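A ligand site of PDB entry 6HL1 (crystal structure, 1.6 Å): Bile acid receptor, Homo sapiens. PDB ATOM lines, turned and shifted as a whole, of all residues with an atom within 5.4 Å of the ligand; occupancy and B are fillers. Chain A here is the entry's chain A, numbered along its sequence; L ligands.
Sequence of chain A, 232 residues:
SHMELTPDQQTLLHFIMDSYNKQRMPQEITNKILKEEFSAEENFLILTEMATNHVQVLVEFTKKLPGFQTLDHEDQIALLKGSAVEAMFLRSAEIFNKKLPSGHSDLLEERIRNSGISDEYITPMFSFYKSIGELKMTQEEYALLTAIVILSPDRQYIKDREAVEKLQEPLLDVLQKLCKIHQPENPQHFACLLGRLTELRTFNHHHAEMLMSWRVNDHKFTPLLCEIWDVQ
A ring nitrogen (ND1) of His 207 sits at hydrogen-bond distance from an oxygen (O1) of the ligand, at 2.8 Å.
The side-chain sulfur (SD) of Met 88 is in hydrogen-bond range of an oxygen (O2) of the ligand, 3.6 Å away.
The guanidinium group (NE) of Arg 91 is in salt-bridge range of an oxygen (O4) of the ligand (3.2 Å).
The side-chain hydroxyl (OH) of Tyr 121 is in hydrogen-bond range of an oxygen (O1) of the ligand (2.8 Å).
An oxygen (O2) of the ligand lies within hydrogen-bond range of the side-chain hydroxyl of Tyr 129 (2.7 Å).
OG of Ser 92 sits at hydrogen-bond distance from O2 of the ligand.
The side-chain hydroxyl (OG) of Ser 92 lies within hydrogen-bond range of the backbone carbonyl oxygen (O) of Met 88 (2.7 Å).
Residues that only touch the ligand: Met 50, Ile 95, His 54, Met 25, Phe 89, Ala 51, Met 210, Ile 112, Trp 214 and Leu 47.
Hydrophobic or aromatic side chains that line the ligand: Met 25, Leu 47, Met 50, Ala 51, His 54, Met 88, Phe 89, Ile 95, Ile 112, Tyr 121, Tyr 129, His 207, Met 210 and Trp 214.
Along chain A the residues within 4 Å of the ligand span positions 25 to 214.
The nearest printed residue that does not touch the ligand is Trp 229 (4.04 Å).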
ATOM      1  N   MET A  25      -4.072   2.240 -16.177  1.00  0.00           N
ATOM      2  CA  MET A  25      -4.269   2.618 -14.798  1.00  0.00           C
ATOM      3  C   MET A  25      -5.049   3.921 -14.676  1.00  0.00           C
ATOM      4  O   MET A  25      -4.768   4.889 -15.399  1.00  0.00           O
ATOM      5  CB  MET A  25      -2.925   2.775 -14.060  1.00  0.00           C
ATOM      6  CG  MET A  25      -3.044   2.699 -12.549  1.00  0.00           C
ATOM      7  SD  MET A  25      -1.780   1.746 -11.659  1.00  0.00           S
ATOM      8  CE  MET A  25      -2.236   0.023 -12.051  1.00  0.00           C
ATOM      9  N   LEU A  47       1.097   1.352  -3.542  1.00  0.00           N
ATOM     10  CA  LEU A  47       1.623   0.241  -4.340  1.00  0.00           C
ATOM     11  C   LEU A  47       0.652  -0.919  -4.353  1.00  0.00           C
ATOM     12  O   LEU A  47       0.476  -1.578  -5.392  1.00  0.00           O
ATOM     13  CB  LEU A  47       2.974  -0.197  -3.776  1.00  0.00           C
ATOM     14  CG  LEU A  47       4.060   0.857  -3.978  1.00  0.00           C
ATOM     15  CD1 LEU A  47       5.322   0.521  -3.208  1.00  0.00           C
ATOM     16  CD2 LEU A  47       4.347   1.049  -5.459  1.00  0.00           C
ATOM     17  N   MET A  50      -2.152   0.016  -6.668  1.00  0.00           N
ATOM     18  CA  MET A  50      -1.728  -0.213  -8.053  1.00  0.00           C
ATOM     19  C   MET A  50      -1.738  -1.700  -8.401  1.00  0.00           C
ATOM     20  O   MET A  50      -2.167  -2.086  -9.493  1.00  0.00           O
ATOM     21  CB  MET A  50      -0.332   0.357  -8.266  1.00  0.00           C
ATOM     22  CG  MET A  50      -0.261   1.862  -8.166  1.00  0.00           C
ATOM     23  SD  MET A  50       1.424   2.430  -8.383  1.00  0.00           S
ATOM     24  CE  MET A  50       1.727   1.783 -10.033  1.00  0.00           C
ATOM     25  N   ALA A  51      -1.232  -2.531  -7.501  1.00  0.00           N
ATOM     26  CA  ALA A  51      -1.171  -3.967  -7.764  1.00  0.00           C
ATOM     27  C   ALA A  51      -2.572  -4.567  -7.911  1.00  0.00           C
ATOM     28  O   ALA A  51      -2.786  -5.462  -8.751  1.00  0.00           O
ATOM     29  CB  ALA A  51      -0.398  -4.656  -6.647  1.00  0.00           C
ATOM     30  N   HIS A  54      -3.731  -3.718 -11.267  1.00  0.00           N
ATOM     31  CA  HIS A  54      -3.060  -4.508 -12.300  1.00  0.00           C
ATOM     32  C   HIS A  54      -3.692  -5.892 -12.433  1.00  0.00           C
ATOM     33  O   HIS A  54      -3.817  -6.412 -13.556  1.00  0.00           O
ATOM     34  CB  HIS A  54      -1.562  -4.609 -12.010  1.00  0.00           C
ATOM     35  CG  HIS A  54      -0.842  -5.574 -12.902  1.00  0.00           C
ATOM     36  ND1 HIS A  54      -0.518  -6.848 -12.490  1.00  0.00           N
ATOM     37  CD2 HIS A  54      -0.422  -5.473 -14.180  1.00  0.00           C
ATOM     38  CE1 HIS A  54       0.072  -7.489 -13.479  1.00  0.00           C
ATOM     39  NE2 HIS A  54       0.136  -6.677 -14.520  1.00  0.00           N
ATOM     40  N   MET A  88       2.997  -9.673 -13.356  1.00  0.00           N
ATOM     41  CA  MET A  88       3.362  -8.426 -12.687  1.00  0.00           C
ATOM     42  C   MET A  88       4.856  -8.154 -12.799  1.00  0.00           C
ATOM     43  O   MET A  88       5.281  -7.000 -12.946  1.00  0.00           O
ATOM     44  CB  MET A  88       2.905  -8.488 -11.224  1.00  0.00           C
ATOM     45  CG  MET A  88       3.256  -7.251 -10.385  1.00  0.00           C
ATOM     46  SD  MET A  88       4.839  -7.426  -9.567  1.00  0.00           S
ATOM     47  CE  MET A  88       4.523  -8.834  -8.493  1.00  0.00           C
ATOM     48  N   PHE A  89       5.692  -9.211 -12.738  1.00  0.00           N
ATOM     49  CA  PHE A  89       7.130  -9.015 -12.904  1.00  0.00           C
ATOM     50  C   PHE A  89       7.449  -8.514 -14.309  1.00  0.00           C
ATOM     51  O   PHE A  89       8.273  -7.614 -14.490  1.00  0.00           O
ATOM     52  CB  PHE A  89       7.894 -10.321 -12.668  1.00  0.00           C
ATOM     53  CG  PHE A  89       7.936 -10.773 -11.241  1.00  0.00           C
ATOM     54  CD1 PHE A  89       7.981  -9.870 -10.207  1.00  0.00           C
ATOM     55  CD2 PHE A  89       7.957 -12.130 -10.946  1.00  0.00           C
ATOM     56  CE1 PHE A  89       8.050 -10.298  -8.896  1.00  0.00           C
ATOM     57  CE2 PHE A  89       8.008 -12.565  -9.639  1.00  0.00           C
ATOM     58  CZ  PHE A  89       8.050 -11.648  -8.618  1.00  0.00           C
ATOM     59  N   ARG A  91       5.494  -6.874 -16.380  1.00  0.00           N
ATOM     60  CA  ARG A  91       5.038  -5.497 -16.501  1.00  0.00           C
ATOM     61  C   ARG A  91       5.986  -4.554 -15.764  1.00  0.00           C
ATOM     62  O   ARG A  91       6.311  -3.468 -16.264  1.00  0.00           O
ATOM     63  CB  ARG A  91       3.602  -5.376 -15.945  1.00  0.00           C
ATOM     64  CG  ARG A  91       2.999  -3.976 -16.040  1.00  0.00           C
ATOM     65  CD  ARG A  91       3.034  -3.393 -17.459  1.00  0.00           C
ATOM     66  NE  ARG A  91       2.454  -2.041 -17.475  1.00  0.00           N
ATOM     67  CZ  ARG A  91       2.723  -1.103 -18.378  1.00  0.00           C
ATOM     68  NH1 ARG A  91       3.591  -1.345 -19.365  1.00  0.00           N
ATOM     69  NH2 ARG A  91       2.141   0.085 -18.290  1.00  0.00           N
ATOM     70  N   SER A  92       6.421  -4.941 -14.576  1.00  0.00           N
ATOM     71  CA  SER A  92       7.401  -4.169 -13.823  1.00  0.00           C
ATOM     72  C   SER A  92       8.669  -3.967 -14.650  1.00  0.00           C
ATOM     73  O   SER A  92       9.209  -2.852 -14.744  1.00  0.00           O
ATOM     74  CB  SER A  92       7.691  -4.874 -12.501  1.00  0.00           C
ATOM     75  OG  SER A  92       6.524  -4.940 -11.728  1.00  0.00           O
ATOM     76  N   ILE A  95       8.003  -1.356 -17.416  1.00  0.00           N
ATOM     77  CA  ILE A  95       7.926   0.020 -16.930  1.00  0.00           C
ATOM     78  C   ILE A  95       9.323   0.568 -16.675  1.00  0.00           C
ATOM     79  O   ILE A  95       9.668   1.676 -17.110  1.00  0.00           O
ATOM     80  CB  ILE A  95       7.048   0.081 -15.676  1.00  0.00           C
ATOM     81  CG1 ILE A  95       5.580  -0.140 -16.054  1.00  0.00           C
ATOM     82  CG2 ILE A  95       7.249   1.396 -14.944  1.00  0.00           C
ATOM     83  CD1 ILE A  95       4.657  -0.349 -14.845  1.00  0.00           C
ATOM     84  N   PHE A  96      10.166  -0.208 -15.996  1.00  0.00           N
ATOM     85  CA  PHE A  96      11.464   0.238 -15.517  1.00  0.00           C
ATOM     86  C   PHE A  96      12.542   0.200 -16.579  1.00  0.00           C
ATOM     87  O   PHE A  96      13.699   0.486 -16.260  1.00  0.00           O
ATOM     88  CB  PHE A  96      11.884  -0.608 -14.317  1.00  0.00           C
ATOM     89  CG  PHE A  96      11.042  -0.369 -13.101  1.00  0.00           C
ATOM     90  CD1 PHE A  96      10.838   0.925 -12.634  1.00  0.00           C
ATOM     91  CD2 PHE A  96      10.463  -1.421 -12.421  1.00  0.00           C
ATOM     92  CE1 PHE A  96      10.065   1.156 -11.516  1.00  0.00           C
ATOM     93  CE2 PHE A  96       9.685  -1.199 -11.311  1.00  0.00           C
ATOM     94  CZ  PHE A  96       9.484   0.097 -10.858  1.00  0.00           C
ATOM     95  N   LEU A 108       8.283   6.116  -8.767  1.00  0.00           N
ATOM     96  CA  LEU A 108       7.748   4.803  -8.440  1.00  0.00           C
ATOM     97  C   LEU A 108       8.821   3.911  -7.833  1.00  0.00           C
ATOM     98  O   LEU A 108       8.569   3.191  -6.859  1.00  0.00           O
ATOM     99  CB  LEU A 108       7.151   4.168  -9.707  1.00  0.00           C
ATOM    100  CG  LEU A 108       6.557   2.782  -9.522  1.00  0.00           C
ATOM    101  CD1 LEU A 108       5.409   2.863  -8.519  1.00  0.00           C
ATOM    102  CD2 LEU A 108       6.097   2.199 -10.851  1.00  0.00           C
ATOM    103  N   ILE A 112       8.831   2.303  -4.044  1.00  0.00           N
ATOM    104  CA  ILE A 112       9.082   0.883  -3.821  1.00  0.00           C
ATOM    105  C   ILE A 112      10.173   0.695  -2.763  1.00  0.00           C
ATOM    106  O   ILE A 112      10.070  -0.188  -1.911  1.00  0.00           O
ATOM    107  CB  ILE A 112       9.442   0.211  -5.152  1.00  0.00           C
ATOM    108  CG1 ILE A 112       8.213   0.199  -6.070  1.00  0.00           C
ATOM    109  CG2 ILE A 112       9.882  -1.207  -4.938  1.00  0.00           C
ATOM    110  CD1 ILE A 112       8.485  -0.214  -7.519  1.00  0.00           C
ATOM    111  N   ILE A 117       9.338  -3.095   2.219  1.00  0.00           N
ATOM    112  CA  ILE A 117       9.957  -4.249   1.577  1.00  0.00           C
ATOM    113  C   ILE A 117      11.461  -4.175   1.771  1.00  0.00           C
ATOM    114  O   ILE A 117      12.094  -3.146   1.518  1.00  0.00           O
ATOM    115  CB  ILE A 117       9.617  -4.302   0.083  1.00  0.00           C
ATOM    116  CG1 ILE A 117       8.100  -4.326  -0.145  1.00  0.00           C
ATOM    117  CG2 ILE A 117      10.246  -5.530  -0.522  1.00  0.00           C
ATOM    118  CD1 ILE A 117       7.718  -4.406  -1.599  1.00  0.00           C
ATOM    119  N   TYR A 121      15.224  -8.067  -0.773  1.00  0.00           N
ATOM    120  CA  TYR A 121      14.350  -8.478  -1.856  1.00  0.00           C
ATOM    121  C   TYR A 121      14.407  -7.534  -3.051  1.00  0.00           C
ATOM    122  O   TYR A 121      14.492  -7.989  -4.192  1.00  0.00           O
ATOM    123  CB  TYR A 121      12.903  -8.574  -1.355  1.00  0.00           C
ATOM    124  CG  TYR A 121      11.882  -9.071  -2.367  1.00  0.00           C
ATOM    125  CD1 TYR A 121      11.658 -10.422  -2.551  1.00  0.00           C
ATOM    126  CD2 TYR A 121      11.110  -8.172  -3.091  1.00  0.00           C
ATOM    127  CE1 TYR A 121      10.708 -10.885  -3.452  1.00  0.00           C
ATOM    128  CE2 TYR A 121      10.155  -8.623  -3.992  1.00  0.00           C
ATOM    129  CZ  TYR A 121       9.961  -9.969  -4.177  1.00  0.00           C
ATOM    130  OH  TYR A 121       9.013 -10.408  -5.082  1.00  0.00           O
ATOM    131  N   ILE A 122      14.399  -6.220  -2.799  1.00  0.00           N
ATOM    132  CA  ILE A 122      14.271  -5.242  -3.872  1.00  0.00           C
ATOM    133  C   ILE A 122      15.495  -5.263  -4.782  1.00  0.00           C
ATOM    134  O   ILE A 122      15.361  -5.293  -6.011  1.00  0.00           O
ATOM    135  CB  ILE A 122      14.039  -3.841  -3.283  1.00  0.00           C
ATOM    136  CG1 ILE A 122      12.754  -3.835  -2.465  1.00  0.00           C
ATOM    137  CG2 ILE A 122      13.987  -2.784  -4.391  1.00  0.00           C
ATOM    138  CD1 ILE A 122      11.523  -3.751  -3.307  1.00  0.00           C
ATOM    139  N   PHE A 126      15.228  -5.785  -8.775  1.00  0.00           N
ATOM    140  CA  PHE A 126      15.543  -4.756  -9.753  1.00  0.00           C
ATOM    141  C   PHE A 126      16.700  -5.188 -10.649  1.00  0.00           C
ATOM    142  O   PHE A 126      16.741  -4.788 -11.819  1.00  0.00           O
ATOM    143  CB  PHE A 126      15.864  -3.435  -9.069  1.00  0.00           C
ATOM    144  CG  PHE A 126      14.648  -2.560  -8.888  1.00  0.00           C
ATOM    145  CD1 PHE A 126      14.334  -1.601  -9.839  1.00  0.00           C
ATOM    146  CD2 PHE A 126      13.803  -2.724  -7.812  1.00  0.00           C
ATOM    147  CE1 PHE A 126      13.215  -0.807  -9.692  1.00  0.00           C
ATOM    148  CE2 PHE A 126      12.681  -1.931  -7.651  1.00  0.00           C
ATOM    149  CZ  PHE A 126      12.386  -0.965  -8.598  1.00  0.00           C
ATOM    150  N   TYR A 129      14.867  -7.174 -13.170  1.00  0.00           N
ATOM    151  CA  TYR A 129      14.212  -6.288 -14.142  1.00  0.00           C
ATOM    152  C   TYR A 129      15.234  -5.717 -15.126  1.00  0.00           C
ATOM    153  O   TYR A 129      14.932  -5.549 -16.314  1.00  0.00           O
ATOM    154  CB  TYR A 129      13.475  -5.162 -13.417  1.00  0.00           C
ATOM    155  CG  TYR A 129      12.367  -5.608 -12.471  1.00  0.00           C
ATOM    156  CD1 TYR A 129      11.778  -6.859 -12.589  1.00  0.00           C
ATOM    157  CD2 TYR A 129      11.890  -4.759 -11.475  1.00  0.00           C
ATOM    158  CE1 TYR A 129      10.758  -7.257 -11.731  1.00  0.00           C
ATOM    159  CE2 TYR A 129      10.880  -5.153 -10.614  1.00  0.00           C
ATOM    160  CZ  TYR A 129      10.310  -6.388 -10.748  1.00  0.00           C
ATOM    161  OH  TYR A 129       9.306  -6.787  -9.909  1.00  0.00           O
ATOM    162  N   HIS A 207       8.709 -13.879  -4.003  1.00  0.00           N
ATOM    163  CA  HIS A 207       7.566 -13.000  -3.714  1.00  0.00           C
ATOM    164  C   HIS A 207       6.726 -13.562  -2.579  1.00  0.00           C
ATOM    165  O   HIS A 207       6.424 -12.854  -1.609  1.00  0.00           O
ATOM    166  CB  HIS A 207       6.728 -12.823  -4.986  1.00  0.00           C
ATOM    167  CG  HIS A 207       5.378 -12.210  -4.764  1.00  0.00           C
ATOM    168  ND1 HIS A 207       5.151 -10.847  -4.844  1.00  0.00           N
ATOM    169  CD2 HIS A 207       4.179 -12.778  -4.501  1.00  0.00           C
ATOM    170  CE1 HIS A 207       3.863 -10.606  -4.667  1.00  0.00           C
ATOM    171  NE2 HIS A 207       3.253 -11.755  -4.444  1.00  0.00           N
ATOM    172  N   MET A 210       8.537 -13.208   0.619  1.00  0.00           N
ATOM    173  CA  MET A 210       8.580 -11.810   1.027  1.00  0.00           C
ATOM    174  C   MET A 210       7.273 -11.394   1.698  1.00  0.00           C
ATOM    175  O   MET A 210       7.273 -10.653   2.684  1.00  0.00           O
ATOM    176  CB  MET A 210       8.860 -10.933  -0.198  1.00  0.00           C
ATOM    177  CG  MET A 210       8.927  -9.436   0.074  1.00  0.00           C
ATOM    178  SD  MET A 210       7.335  -8.574  -0.098  1.00  0.00           S
ATOM    179  CE  MET A 210       7.000  -8.770  -1.839  1.00  0.00           C
ATOM    180  N   TRP A 214       6.144  -8.705   4.853  1.00  0.00           N
ATOM    181  CA  TRP A 214       5.859  -7.345   4.407  1.00  0.00           C
ATOM    182  C   TRP A 214       4.679  -6.789   5.190  1.00  0.00           C
ATOM    183  O   TRP A 214       3.530  -7.204   4.966  1.00  0.00           O
ATOM    184  CB  TRP A 214       5.581  -7.327   2.903  1.00  0.00           C
ATOM    185  CG  TRP A 214       5.415  -5.958   2.308  1.00  0.00           C
ATOM    186  CD1 TRP A 214       5.772  -4.773   2.881  1.00  0.00           C
ATOM    187  CD2 TRP A 214       4.857  -5.650   1.029  1.00  0.00           C
ATOM    188  NE1 TRP A 214       5.443  -3.732   2.038  1.00  0.00           N
ATOM    189  CE2 TRP A 214       4.890  -4.245   0.894  1.00  0.00           C
ATOM    190  CE3 TRP A 214       4.312  -6.408  -0.009  1.00  0.00           C
ATOM    191  CZ2 TRP A 214       4.419  -3.583  -0.242  1.00  0.00           C
ATOM    192  CZ3 TRP A 214       3.847  -5.759  -1.146  1.00  0.00           C
ATOM    193  CH2 TRP A 214       3.895  -4.357  -1.242  1.00  0.00           C
ATOM    194  N   TRP A 229      -2.634 -13.367  -4.084  1.00  0.00           N
ATOM    195  CA  TRP A 229      -1.307 -13.586  -3.513  1.00  0.00           C
ATOM    196  C   TRP A 229      -1.317 -14.571  -2.358  1.00  0.00           C
ATOM    197  O   TRP A 229      -0.252 -14.853  -1.786  1.00  0.00           O
ATOM    198  CB  TRP A 229      -0.706 -12.256  -3.059  1.00  0.00           C
ATOM    199  CG  TRP A 229      -0.219 -11.373  -4.188  1.00  0.00           C
ATOM    200  CD1 TRP A 229      -0.168 -11.699  -5.509  1.00  0.00           C
ATOM    201  CD2 TRP A 229       0.270 -10.041  -4.065  1.00  0.00           C
ATOM    202  NE1 TRP A 229       0.332 -10.617  -6.230  1.00  0.00           N
ATOM    203  CE2 TRP A 229       0.613  -9.603  -5.364  1.00  0.00           C
ATOM    204  CE3 TRP A 229       0.473  -9.173  -2.984  1.00  0.00           C
ATOM    205  CZ2 TRP A 229       1.134  -8.329  -5.611  1.00  0.00           C
ATOM    206  CZ3 TRP A 229       0.985  -7.903  -3.233  1.00  0.00           C
ATOM    207  CH2 TRP A 229       1.303  -7.491  -4.524  1.00  0.00           C
HETATM  208  C1  LIG L   1       5.165  -5.565  -4.800  1.00  0.00           C
HETATM  209  C2  LIG L   1       5.236  -7.012  -5.330  1.00  0.00           C
HETATM  210  C3  LIG L   1       6.706  -7.419  -5.384  1.00  0.00           C
HETATM  211  O1  LIG L   1       6.850  -8.826  -5.722  1.00  0.00           O
HETATM  212  C4  LIG L   1       7.429  -6.526  -6.402  1.00  0.00           C
HETATM  213  C5  LIG L   1       7.374  -5.055  -5.939  1.00  0.00           C
HETATM  214  C6  LIG L   1       8.134  -4.088  -6.870  1.00  0.00           C
HETATM  215  C7  LIG L   1       7.432  -3.830  -8.202  1.00  0.00           C
HETATM  216  O2  LIG L   1       7.521  -5.014  -9.032  1.00  0.00           O
HETATM  217  C8  LIG L   1       5.954  -3.425  -7.969  1.00  0.00           C
HETATM  218  C9  LIG L   1       5.216  -4.479  -7.123  1.00  0.00           C
HETATM  219  C10 LIG L   1       5.906  -4.599  -5.742  1.00  0.00           C
HETATM  220  C11 LIG L   1       3.732  -4.088  -6.980  1.00  0.00           C
HETATM  221  C12 LIG L   1       3.052  -3.835  -8.352  1.00  0.00           C
HETATM  222  C13 LIG L   1       3.820  -2.784  -9.178  1.00  0.00           C
HETATM  223  C14 LIG L   1       5.237  -3.256  -9.321  1.00  0.00           C
HETATM  224  C15 LIG L   1       5.801  -2.165 -10.195  1.00  0.00           C
HETATM  225  C16 LIG L   1       4.719  -1.989 -11.267  1.00  0.00           C
HETATM  226  C17 LIG L   1       3.483  -2.728 -10.689  1.00  0.00           C
HETATM  227  C18 LIG L   1       3.740  -1.383  -8.532  1.00  0.00           C
HETATM  228  C19 LIG L   1       5.913  -3.209  -5.066  1.00  0.00           C
HETATM  229  C20 LIG L   1       2.222  -1.943 -11.105  1.00  0.00           C
HETATM  230  C21 LIG L   1       0.916  -2.512 -10.521  1.00  0.00           C
HETATM  231  C22 LIG L   1       2.105  -1.971 -12.649  1.00  0.00           C
HETATM  232  C23 LIG L   1       1.112  -0.876 -13.053  1.00  0.00           C
HETATM  233  O3  LIG L   1       1.234   0.247 -15.127  1.00  0.00           O
HETATM  234  C24 LIG L   1       0.889  -0.803 -14.555  1.00  0.00           C
HETATM  235  O4  LIG L   1       0.342  -1.786 -15.091  1.00  0.00           O
